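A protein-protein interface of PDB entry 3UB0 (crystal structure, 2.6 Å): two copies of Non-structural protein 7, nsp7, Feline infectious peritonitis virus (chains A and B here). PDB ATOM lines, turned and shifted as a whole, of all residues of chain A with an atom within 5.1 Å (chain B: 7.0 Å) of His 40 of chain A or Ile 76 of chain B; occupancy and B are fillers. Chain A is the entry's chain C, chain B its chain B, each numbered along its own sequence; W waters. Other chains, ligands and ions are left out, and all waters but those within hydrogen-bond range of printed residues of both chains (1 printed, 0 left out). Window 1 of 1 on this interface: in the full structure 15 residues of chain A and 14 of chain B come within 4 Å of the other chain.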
ATOM      1  N   ASN A  14      -2.961 -11.844  -2.962  1.00  0.00           N
ATOM      2  CA  ASN A  14      -3.457 -13.213  -2.884  1.00  0.00           C
ATOM      3  C   ASN A  14      -2.318 -14.252  -2.988  1.00  0.00           C
ATOM      4  O   ASN A  14      -2.283 -15.213  -2.213  1.00  0.00           O
ATOM      5  CB  ASN A  14      -4.543 -13.378  -3.941  1.00  0.00           C
ATOM      6  CG  ASN A  14      -4.832 -14.767  -4.392  1.00  0.00           C
ATOM      7  OD1 ASN A  14      -4.824 -15.065  -5.585  1.00  0.00           O
ATOM      8  ND2 ASN A  14      -5.142 -15.625  -3.462  1.00  0.00           N
ATOM      9  N   VAL A  15      -1.373 -14.014  -3.914  1.00  0.00           N
ATOM     10  CA  VAL A  15      -0.182 -14.832  -4.151  1.00  0.00           C
ATOM     11  C   VAL A  15       0.703 -14.855  -2.881  1.00  0.00           C
ATOM     12  O   VAL A  15       1.121 -15.931  -2.456  1.00  0.00           O
ATOM     13  CB  VAL A  15       0.569 -14.321  -5.408  1.00  0.00           C
ATOM     14  CG1 VAL A  15       1.943 -14.964  -5.562  1.00  0.00           C
ATOM     15  CG2 VAL A  15      -0.261 -14.564  -6.652  1.00  0.00           C
ATOM     16  N   LEU A  18      -1.157 -16.932  -0.107  1.00  0.00           N
ATOM     17  CA  LEU A  18      -1.008 -18.371  -0.303  1.00  0.00           C
ATOM     18  C   LEU A  18       0.379 -18.867   0.055  1.00  0.00           C
ATOM     19  O   LEU A  18       0.492 -19.939   0.643  1.00  0.00           O
ATOM     20  CB  LEU A  18      -1.444 -18.856  -1.697  1.00  0.00           C
ATOM     21  CG  LEU A  18      -1.667 -20.386  -1.784  1.00  0.00           C
ATOM     22  CD1 LEU A  18      -3.009 -20.809  -1.152  1.00  0.00           C
ATOM     23  CD2 LEU A  18      -1.492 -20.897  -3.197  1.00  0.00           C
ATOM     24  N   GLY A  19       1.396 -18.077  -0.270  1.00  0.00           N
ATOM     25  CA  GLY A  19       2.789 -18.365   0.062  1.00  0.00           C
ATOM     26  C   GLY A  19       2.995 -18.432   1.565  1.00  0.00           C
ATOM     27  O   GLY A  19       3.578 -19.391   2.068  1.00  0.00           O
ATOM     28  N   CYS A  36      -8.205 -22.978   0.738  1.00  0.00           N
ATOM     29  CA  CYS A  36      -7.189 -21.934   0.511  1.00  0.00           C
ATOM     30  C   CYS A  36      -6.745 -21.877  -0.910  1.00  0.00           C
ATOM     31  O   CYS A  36      -6.761 -20.798  -1.497  1.00  0.00           O
ATOM     32  CB  CYS A  36      -5.989 -22.139   1.421  1.00  0.00           C
ATOM     33  SG  CYS A  36      -6.332 -21.797   3.135  1.00  0.00           S
ATOM     34  N   VAL A  37      -6.267 -23.030  -1.433  1.00  0.00           N
ATOM     35  CA  VAL A  37      -5.793 -23.204  -2.807  1.00  0.00           C
ATOM     36  C   VAL A  37      -6.932 -22.849  -3.775  1.00  0.00           C
ATOM     37  O   VAL A  37      -6.695 -22.128  -4.748  1.00  0.00           O
ATOM     38  CB  VAL A  37      -5.193 -24.619  -3.063  1.00  0.00           C
ATOM     39  CG1 VAL A  37      -4.768 -24.779  -4.515  1.00  0.00           C
ATOM     40  CG2 VAL A  37      -4.004 -24.878  -2.151  1.00  0.00           C
ATOM     41  N   GLY A  38      -8.147 -23.290  -3.439  1.00  0.00           N
ATOM     42  CA  GLY A  38      -9.353 -23.012  -4.195  1.00  0.00           C
ATOM     43  C   GLY A  38      -9.602 -21.531  -4.361  1.00  0.00           C
ATOM     44  O   GLY A  38      -9.748 -21.055  -5.489  1.00  0.00           O
ATOM     45  N   LEU A  39      -9.592 -20.789  -3.248  1.00  0.00           N
ATOM     46  CA  LEU A  39      -9.799 -19.340  -3.231  1.00  0.00           C
ATOM     47  C   LEU A  39      -8.724 -18.602  -4.031  1.00  0.00           C
ATOM     48  O   LEU A  39      -9.058 -17.736  -4.838  1.00  0.00           O
ATOM     49  CB  LEU A  39      -9.840 -18.786  -1.786  1.00  0.00           C
ATOM     50  CG  LEU A  39     -11.109 -18.988  -0.982  1.00  0.00           C
ATOM     51  CD1 LEU A  39     -10.852 -18.650   0.470  1.00  0.00           C
ATOM     52  CD2 LEU A  39     -12.274 -18.168  -1.539  1.00  0.00           C
ATOM     53  N   HIS A  40      -7.448 -18.972  -3.832  1.00  0.00           N
ATOM     54  CA  HIS A  40      -6.307 -18.389  -4.523  1.00  0.00           C
ATOM     55  C   HIS A  40      -6.429 -18.534  -6.034  1.00  0.00           C
ATOM     56  O   HIS A  40      -6.294 -17.549  -6.749  1.00  0.00           O
ATOM     57  CB  HIS A  40      -4.982 -18.997  -3.998  1.00  0.00           C
ATOM     58  CG  HIS A  40      -3.802 -18.775  -4.901  1.00  0.00           C
ATOM     59  ND1 HIS A  40      -3.498 -19.676  -5.904  1.00  0.00           N
ATOM     60  CD2 HIS A  40      -2.910 -17.759  -4.945  1.00  0.00           C
ATOM     61  CE1 HIS A  40      -2.416 -19.200  -6.504  1.00  0.00           C
ATOM     62  NE2 HIS A  40      -2.037 -18.045  -5.978  1.00  0.00           N
ATOM     63  N   ASN A  41      -6.666 -19.772  -6.505  1.00  0.00           N
ATOM     64  CA  ASN A  41      -6.810 -20.111  -7.923  1.00  0.00           C
ATOM     65  C   ASN A  41      -7.989 -19.404  -8.564  1.00  0.00           C
ATOM     66  O   ASN A  41      -7.853 -18.928  -9.686  1.00  0.00           O
ATOM     67  CB  ASN A  41      -6.906 -21.624  -8.123  1.00  0.00           C
ATOM     68  CG  ASN A  41      -5.637 -22.365  -7.799  1.00  0.00           C
ATOM     69  OD1 ASN A  41      -4.560 -21.774  -7.537  1.00  0.00           O
ATOM     70  ND2 ASN A  41      -5.732 -23.687  -7.838  1.00  0.00           N
ATOM     71  N   GLU A  42      -9.131 -19.319  -7.849  1.00  0.00           N
ATOM     72  CA  GLU A  42     -10.335 -18.631  -8.308  1.00  0.00           C
ATOM     73  C   GLU A  42     -10.051 -17.130  -8.463  1.00  0.00           C
ATOM     74  O   GLU A  42     -10.465 -16.550  -9.457  1.00  0.00           O
ATOM     75  CB  GLU A  42     -11.504 -18.868  -7.339  1.00  0.00           C
ATOM     76  CG  GLU A  42     -12.222 -20.200  -7.489  1.00  0.00           C
ATOM     77  CD  GLU A  42     -12.948 -20.710  -6.248  1.00  0.00           C
ATOM     78  OE1 GLU A  42     -13.584 -19.902  -5.530  1.00  0.00           O
ATOM     79  OE2 GLU A  42     -12.891 -21.937  -6.001  1.00  0.00           O
ATOM     80  N   ILE A  43      -9.316 -16.512  -7.503  1.00  0.00           N
ATOM     81  CA  ILE A  43      -8.945 -15.089  -7.566  1.00  0.00           C
ATOM     82  C   ILE A  43      -8.173 -14.790  -8.851  1.00  0.00           C
ATOM     83  O   ILE A  43      -8.528 -13.854  -9.565  1.00  0.00           O
ATOM     84  CB  ILE A  43      -8.176 -14.612  -6.297  1.00  0.00           C
ATOM     85  CG1 ILE A  43      -9.128 -14.484  -5.109  1.00  0.00           C
ATOM     86  CG2 ILE A  43      -7.425 -13.274  -6.539  1.00  0.00           C
ATOM     87  CD1 ILE A  43      -8.408 -14.353  -3.731  1.00  0.00           C
ATOM     88  N   ASN A  44      -7.146 -15.614  -9.146  1.00  0.00           N
ATOM     89  CA  ASN A  44      -6.273 -15.454 -10.310  1.00  0.00           C
ATOM     90  C   ASN A  44      -6.942 -15.640 -11.660  1.00  0.00           C
ATOM     91  O   ASN A  44      -6.438 -15.113 -12.656  1.00  0.00           O
ATOM     92  CB  ASN A  44      -5.015 -16.303 -10.175  1.00  0.00           C
ATOM     93  CG  ASN A  44      -4.166 -15.950  -8.986  1.00  0.00           C
ATOM     94  OD1 ASN A  44      -4.056 -14.799  -8.570  1.00  0.00           O
ATOM     95  ND2 ASN A  44      -3.541 -16.929  -8.409  1.00  0.00           N
ATOM     96  N   LEU A  59      -9.871 -15.180   2.160  1.00  0.00           N
ATOM     97  CA  LEU A  59      -8.498 -15.660   2.329  1.00  0.00           C
ATOM     98  C   LEU A  59      -7.806 -14.957   3.488  1.00  0.00           C
ATOM     99  O   LEU A  59      -7.157 -15.625   4.292  1.00  0.00           O
ATOM    100  CB  LEU A  59      -7.704 -15.527   1.025  1.00  0.00           C
ATOM    101  CG  LEU A  59      -6.460 -16.441   0.828  1.00  0.00           C
ATOM    102  CD1 LEU A  59      -6.767 -17.934   0.912  1.00  0.00           C
ATOM    103  CD2 LEU A  59      -5.822 -16.168  -0.481  1.00  0.00           C
ATOM    104  N   VAL B  16      11.590 -25.953  -8.806  1.00  0.00           N
ATOM    105  CA  VAL B  16      10.126 -26.075  -8.789  1.00  0.00           C
ATOM    106  C   VAL B  16       9.511 -25.679 -10.126  1.00  0.00           C
ATOM    107  O   VAL B  16       8.628 -26.397 -10.612  1.00  0.00           O
ATOM    108  CB  VAL B  16       9.458 -25.419  -7.555  1.00  0.00           C
ATOM    109  CG1 VAL B  16       7.939 -25.516  -7.632  1.00  0.00           C
ATOM    110  CG2 VAL B  16       9.970 -26.063  -6.264  1.00  0.00           C
ATOM    111  N   LEU B  53       6.251  -9.708  -8.701  1.00  0.00           N
ATOM    112  CA  LEU B  53       4.977 -10.344  -8.367  1.00  0.00           C
ATOM    113  C   LEU B  53       4.069 -10.440  -9.582  1.00  0.00           C
ATOM    114  O   LEU B  53       3.373 -11.443  -9.748  1.00  0.00           O
ATOM    115  CB  LEU B  53       4.275  -9.603  -7.208  1.00  0.00           C
ATOM    116  CG  LEU B  53       4.810  -9.818  -5.776  1.00  0.00           C
ATOM    117  CD1 LEU B  53       4.115  -8.893  -4.826  1.00  0.00           C
ATOM    118  CD2 LEU B  53       4.572 -11.250  -5.269  1.00  0.00           C
ATOM    119  N   LEU B  56       5.325 -13.326 -11.582  1.00  0.00           N
ATOM    120  CA  LEU B  56       4.993 -14.564 -10.867  1.00  0.00           C
ATOM    121  C   LEU B  56       3.492 -14.890 -11.098  1.00  0.00           C
ATOM    122  O   LEU B  56       3.125 -16.047 -11.340  1.00  0.00           O
ATOM    123  CB  LEU B  56       5.270 -14.368  -9.363  1.00  0.00           C
ATOM    124  CG  LEU B  56       5.683 -15.544  -8.454  1.00  0.00           C
ATOM    125  CD1 LEU B  56       5.318 -15.270  -7.037  1.00  0.00           C
ATOM    126  CD2 LEU B  56       5.180 -16.966  -8.896  1.00  0.00           C
ATOM    127  N   LEU B  57       2.641 -13.847 -11.074  1.00  0.00           N
ATOM    128  CA  LEU B  57       1.207 -13.934 -11.337  1.00  0.00           C
ATOM    129  C   LEU B  57       0.953 -14.432 -12.761  1.00  0.00           C
ATOM    130  O   LEU B  57      -0.008 -15.179 -12.974  1.00  0.00           O
ATOM    131  CB  LEU B  57       0.573 -12.555 -11.131  1.00  0.00           C
ATOM    132  CG  LEU B  57      -0.930 -12.446 -10.997  1.00  0.00           C
ATOM    133  CD1 LEU B  57      -1.426 -13.223  -9.803  1.00  0.00           C
ATOM    134  CD2 LEU B  57      -1.333 -10.990 -10.882  1.00  0.00           C
ATOM    135  N   ILE B  60       1.764 -18.205 -12.753  1.00  0.00           N
ATOM    136  CA  ILE B  60       0.618 -18.861 -12.104  1.00  0.00           C
ATOM    137  C   ILE B  60      -0.557 -18.977 -13.121  1.00  0.00           C
ATOM    138  O   ILE B  60      -1.069 -20.073 -13.326  1.00  0.00           O
ATOM    139  CB  ILE B  60       0.243 -18.115 -10.796  1.00  0.00           C
ATOM    140  CG1 ILE B  60       1.290 -18.418  -9.684  1.00  0.00           C
ATOM    141  CG2 ILE B  60      -1.181 -18.440 -10.340  1.00  0.00           C
ATOM    142  CD1 ILE B  60       1.367 -17.350  -8.551  1.00  0.00           C
ATOM    143  N   LEU B  64      -2.408 -22.436 -14.361  1.00  0.00           N
ATOM    144  CA  LEU B  64      -3.841 -22.563 -14.076  1.00  0.00           C
ATOM    145  C   LEU B  64      -4.680 -22.679 -15.358  1.00  0.00           C
ATOM    146  O   LEU B  64      -5.778 -23.238 -15.315  1.00  0.00           O
ATOM    147  CB  LEU B  64      -4.353 -21.441 -13.163  1.00  0.00           C
ATOM    148  CG  LEU B  64      -3.794 -21.382 -11.720  1.00  0.00           C
ATOM    149  CD1 LEU B  64      -4.323 -20.137 -10.975  1.00  0.00           C
ATOM    150  CD2 LEU B  64      -4.133 -22.650 -10.938  1.00  0.00           C
ATOM    151  N   CYS B  70      -4.559 -26.641  -9.846  1.00  0.00           N
ATOM    152  CA  CYS B  70      -3.140 -26.817  -9.536  1.00  0.00           C
ATOM    153  C   CYS B  70      -2.753 -26.112  -8.227  1.00  0.00           C
ATOM    154  O   CYS B  70      -3.149 -24.964  -7.999  1.00  0.00           O
ATOM    155  CB  CYS B  70      -2.301 -26.306 -10.700  1.00  0.00           C
ATOM    156  SG  CYS B  70      -0.562 -26.802 -10.647  1.00  0.00           S
ATOM    157  N   ASP B  71      -2.000 -26.813  -7.358  1.00  0.00           N
ATOM    158  CA  ASP B  71      -1.478 -26.250  -6.119  1.00  0.00           C
ATOM    159  C   ASP B  71      -0.093 -25.701  -6.455  1.00  0.00           C
ATOM    160  O   ASP B  71       0.869 -26.454  -6.521  1.00  0.00           O
ATOM    161  CB  ASP B  71      -1.407 -27.312  -5.001  1.00  0.00           C
ATOM    162  CG  ASP B  71      -0.812 -26.829  -3.678  1.00  0.00           C
ATOM    163  OD1 ASP B  71      -0.834 -27.606  -2.704  1.00  0.00           O
ATOM    164  OD2 ASP B  71      -0.296 -25.683  -3.631  1.00  0.00           O
ATOM    165  N   LEU B  72      -0.009 -24.392  -6.667  1.00  0.00           N
ATOM    166  CA  LEU B  72       1.220 -23.683  -7.051  1.00  0.00           C
ATOM    167  C   LEU B  72       1.995 -23.001  -5.893  1.00  0.00           C
ATOM    168  O   LEU B  72       2.946 -22.267  -6.158  1.00  0.00           O
ATOM    169  CB  LEU B  72       0.877 -22.670  -8.171  1.00  0.00           C
ATOM    170  CG  LEU B  72       0.448 -23.318  -9.486  1.00  0.00           C
ATOM    171  CD1 LEU B  72      -0.475 -22.431 -10.255  1.00  0.00           C
ATOM    172  CD2 LEU B  72       1.634 -23.683 -10.314  1.00  0.00           C
ATOM    173  N   SER B  73       1.634 -23.311  -4.624  1.00  0.00           N
ATOM    174  CA  SER B  73       2.233 -22.779  -3.390  1.00  0.00           C
ATOM    175  C   SER B  73       3.732 -22.978  -3.263  1.00  0.00           C
ATOM    176  O   SER B  73       4.403 -22.140  -2.646  1.00  0.00           O
ATOM    177  CB  SER B  73       1.496 -23.265  -2.137  1.00  0.00           C
ATOM    178  OG  SER B  73       1.437 -24.677  -2.029  1.00  0.00           O
ATOM    179  N   ASP B  74       4.265 -24.035  -3.865  1.00  0.00           N
ATOM    180  CA  ASP B  74       5.696 -24.324  -3.826  1.00  0.00           C
ATOM    181  C   ASP B  74       6.488 -23.425  -4.752  1.00  0.00           C
ATOM    182  O   ASP B  74       7.625 -23.097  -4.431  1.00  0.00           O
ATOM    183  CB  ASP B  74       5.961 -25.815  -4.075  1.00  0.00           C
ATOM    184  CG  ASP B  74       5.472 -26.694  -2.924  1.00  0.00           C
ATOM    185  OD1 ASP B  74       4.729 -27.660  -3.193  1.00  0.00           O
ATOM    186  OD2 ASP B  74       5.758 -26.354  -1.744  1.00  0.00           O
ATOM    187  N   LEU B  75       5.869 -23.006  -5.885  1.00  0.00           N
ATOM    188  CA  LEU B  75       6.409 -22.106  -6.908  1.00  0.00           C
ATOM    189  C   LEU B  75       6.570 -20.758  -6.239  1.00  0.00           C
ATOM    190  O   LEU B  75       7.656 -20.173  -6.300  1.00  0.00           O
ATOM    191  CB  LEU B  75       5.390 -21.991  -8.056  1.00  0.00           C
ATOM    192  CG  LEU B  75       5.838 -21.863  -9.531  1.00  0.00           C
ATOM    193  CD1 LEU B  75       5.060 -20.797 -10.249  1.00  0.00           C
ATOM    194  CD2 LEU B  75       7.347 -21.772  -9.725  1.00  0.00           C
ATOM    195  N   ILE B  76       5.504 -20.299  -5.521  1.00  0.00           N
ATOM    196  CA  ILE B  76       5.512 -19.047  -4.773  1.00  0.00           C
ATOM    197  C   ILE B  76       6.636 -19.088  -3.694  1.00  0.00           C
ATOM    198  O   ILE B  76       7.442 -18.155  -3.623  1.00  0.00           O
ATOM    199  CB  ILE B  76       4.120 -18.758  -4.164  1.00  0.00           C
ATOM    200  CG1 ILE B  76       3.040 -18.578  -5.247  1.00  0.00           C
ATOM    201  CG2 ILE B  76       4.189 -17.549  -3.218  1.00  0.00           C
ATOM    202  CD1 ILE B  76       1.582 -18.781  -4.738  1.00  0.00           C
ATOM    203  N   GLU B  77       6.698 -20.180  -2.886  1.00  0.00           N
ATOM    204  CA  GLU B  77       7.717 -20.367  -1.856  1.00  0.00           C
ATOM    205  C   GLU B  77       9.131 -20.239  -2.416  1.00  0.00           C
ATOM    206  O   GLU B  77       9.928 -19.471  -1.869  1.00  0.00           O
ATOM    207  CB  GLU B  77       7.568 -21.738  -1.189  1.00  0.00           C
ATOM    208  CG  GLU B  77       6.576 -21.761  -0.051  1.00  0.00           C
ATOM    209  CD  GLU B  77       6.731 -22.929   0.897  1.00  0.00           C
ATOM    210  OE1 GLU B  77       5.696 -23.494   1.305  1.00  0.00           O
ATOM    211  OE2 GLU B  77       7.873 -23.215   1.319  1.00  0.00           O
ATOM    212  N   SER B  78       9.428 -20.978  -3.502  1.00  0.00           N
ATOM    213  CA  SER B  78      10.732 -21.019  -4.172  1.00  0.00           C
ATOM    214  C   SER B  78      11.152 -19.646  -4.670  1.00  0.00           C
ATOM    215  O   SER B  78      12.324 -19.297  -4.505  1.00  0.00           O
ATOM    216  CB  SER B  78      10.763 -22.066  -5.290  1.00  0.00           C
ATOM    217  OG  SER B  78      10.073 -21.650  -6.453  1.00  0.00           O
ATOM    218  N   TYR B  79      10.205 -18.854  -5.233  1.00  0.00           N
ATOM    219  CA  TYR B  79      10.530 -17.486  -5.646  1.00  0.00           C
ATOM    220  C   TYR B  79      10.900 -16.593  -4.454  1.00  0.00           C
ATOM    221  O   TYR B  79      11.956 -15.973  -4.504  1.00  0.00           O
ATOM    222  CB  TYR B  79       9.500 -16.869  -6.611  1.00  0.00           C
ATOM    223  CG  TYR B  79       9.736 -17.336  -8.031  1.00  0.00           C
ATOM    224  CD1 TYR B  79      10.813 -16.857  -8.772  1.00  0.00           C
ATOM    225  CD2 TYR B  79       8.953 -18.341  -8.594  1.00  0.00           C
ATOM    226  CE1 TYR B  79      11.085 -17.338 -10.051  1.00  0.00           C
ATOM    227  CE2 TYR B  79       9.208 -18.821  -9.877  1.00  0.00           C
ATOM    228  CZ  TYR B  79      10.271 -18.311 -10.607  1.00  0.00           C
ATOM    229  OH  TYR B  79      10.536 -18.761 -11.881  1.00  0.00           O
ATOM    230  N   PHE B  80      10.142 -16.643  -3.336  1.00  0.00           N
ATOM    231  CA  PHE B  80      10.495 -15.910  -2.095  1.00  0.00           C
ATOM    232  C   PHE B  80      11.850 -16.326  -1.518  1.00  0.00           C
ATOM    233  O   PHE B  80      12.561 -15.494  -0.969  1.00  0.00           O
ATOM    234  CB  PHE B  80       9.395 -16.028  -1.024  1.00  0.00           C
ATOM    235  CG  PHE B  80       8.354 -14.972  -1.231  1.00  0.00           C
ATOM    236  CD1 PHE B  80       8.514 -13.699  -0.686  1.00  0.00           C
ATOM    237  CD2 PHE B  80       7.256 -15.208  -2.059  1.00  0.00           C
ATOM    238  CE1 PHE B  80       7.576 -12.684  -0.935  1.00  0.00           C
ATOM    239  CE2 PHE B  80       6.323 -14.192  -2.320  1.00  0.00           C
ATOM    240  CZ  PHE B  80       6.496 -12.933  -1.764  1.00  0.00           C
ATOM    241  N   GLU B  81      12.205 -17.599  -1.677  1.00  0.00           N
ATOM    242  CA  GLU B  81      13.449 -18.203  -1.205  1.00  0.00           C
ATOM    243  C   GLU B  81      14.654 -17.975  -2.111  1.00  0.00           C
ATOM    244  O   GLU B  81      15.774 -18.078  -1.636  1.00  0.00           O
ATOM    245  CB  GLU B  81      13.244 -19.698  -1.045  1.00  0.00           C
ATOM    246  CG  GLU B  81      12.805 -20.083   0.351  1.00  0.00           C
ATOM    247  CD  GLU B  81      12.636 -21.570   0.573  1.00  0.00           C
ATOM    248  OE1 GLU B  81      13.282 -22.376  -0.143  1.00  0.00           O
ATOM    249  OE2 GLU B  81      11.855 -21.927   1.486  1.00  0.00           O
ATOM    250  N   LEU B  86      12.745 -10.206  -3.270  1.00  0.00           N
ATOM    251  CA  LEU B  86      11.599 -10.669  -2.470  1.00  0.00           C
ATOM    252  C   LEU B  86      11.943 -10.902  -1.001  1.00  0.00           C
ATOM    253  O   LEU B  86      11.084 -11.316  -0.205  1.00  0.00           O
ATOM    254  CB  LEU B  86      10.979 -11.920  -3.101  1.00  0.00           C
ATOM    255  CG  LEU B  86       9.650 -11.728  -3.863  1.00  0.00           C
ATOM    256  CD1 LEU B  86       9.445 -10.309  -4.365  1.00  0.00           C
ATOM    257  CD2 LEU B  86       9.510 -12.740  -4.983  1.00  0.00           C
HETATM  258  O   HOH W   1      -2.269 -22.622  -6.210  1.00  0.00           O
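Val 15 of chain A touches Leu 56 of chain B (CG1 to CD1, 3.7 Å).
Val 15 of chain A touches Ile 60 of chain B.
Ile 76 of chain B touches Val 15 of chain A (CG2 to O, 3.6 Å).
Leu 18 of chain A touches Ser 73 of chain B (CD2 to CB, 3.96 Å).
Ile 76 of chain B touches Gly 19 of chain A (CG2 to CA, 3.7 Å).
Val 37 of chain A touches Cys 70 of chain B.
Asp 71 of chain B touches Val 37 of chain A.
NE2 of His 40 of chain A touches CD1 of Ile 76 of chain B (3.9 Å).
Leu 64 of chain B touches Asn 41 of chain A (CD2 to CG, 3.5 Å).
Leu 64 of chain B touches Asn 44 of chain A (CD1 to CB, 3.98 Å).
Of chain B, only Ile 76 comes within 4 Å of His 40 of chain A.
Ile 76 of chain B touches three residues of chain A.
Printed residues of chain A within 4 Å of Ile 60 of chain B: Val 15 and Asn 44.
Printed residues of chain B within 4 Å of Asn 44 of chain A: Leu 57 (3.3 Å), Ile 60 (3.4 Å) and Leu 64 (3.98 Å).
Printed residues of chain B within 4 Å of Asn 41 of chain A: Leu 64 (3.5 Å) and Cys 70 (2.9 Å).
Printed residues of chain B within 4 Å of Val 37 of chain A: Cys 70 (3.8 Å) and Asp 71 (3.9 Å).
Printed residues of chain B within 4 Å of Gly 19 of chain A: Ile 76.
Leu 86 of chain B touches none of the printed residues of chain A.
Asn 14 of chain A touches none of the printed residues of chain B.
The nearest residue of chain B that does not touch His 40 of chain A is Ile 60 of chain B (4.1 Å).
The nearest residue of chain A that does not touch Ile 76 of chain B is Leu 18 of chain A (4.04 Å).
The side-chain carboxylate of Asp 71 of chain B lies within hydrogen-bond range of the side-chain hydroxyl of Ser 73 of chain B (2.6 Å).
The side-chain amide oxygen of Asn 14 of chain A sits close to the backbone carbonyl oxygen of His 40 of chain A (3.1 Å).
The side-chain amide oxygen (OD1) of Asn 44 of chain A lies close to the side-chain amide oxygen (OD1) of Asn 14 of chain A (3.1 Å).
ND1 of His 40 of chain A is in hydrogen-bond range of OD1 of Asn 41 of chain A, 2.9 Å away.
The side-chain amide nitrogen of Asn 44 of chain A lies within hydrogen-bond range of a ring nitrogen (NE2) of His 40 of chain A (3.1 Å).
Of the 19 printed residues of chain B, 8 touch a printed residue of chain A.
Hydrophobic or aromatic side chains of chain B that line the printed part of chain A: Leu 56, Leu 57, Ile 60, Leu 64 and Ile 76.
Along chain B the printed residues that touch a printed residue of chain A span positions 56 to 76.
Hydrophobic or aromatic side chains of chain A that line the printed part of chain B: Val 15, Leu 18, Val 37 and His 40.
Among the printed residues, 14 pairs touch across the chains.
Among the printed residues, no Asp or Glu carboxylate lies within 4 Å of a Lys or Arg side-chain nitrogen of the other chain.
O of Cys 70 of chain B is in hydrogen-bond range of ND2 of Asn 41 of chain A, at 2.9 Å.
No position is printed for both chains.
Water W1 lies within hydrogen-bond range of the side-chain amide oxygen (OD1) of Asn 41 of chain A (2.8 Å), the backbone NH (N) of Leu 72 of chain B (2.9 Å), the backbone carbonyl oxygen (O) of Cys 70 of chain B (3.1 Å) and a ring nitrogen (ND1) of His 40 of chain A (3.2 Å).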
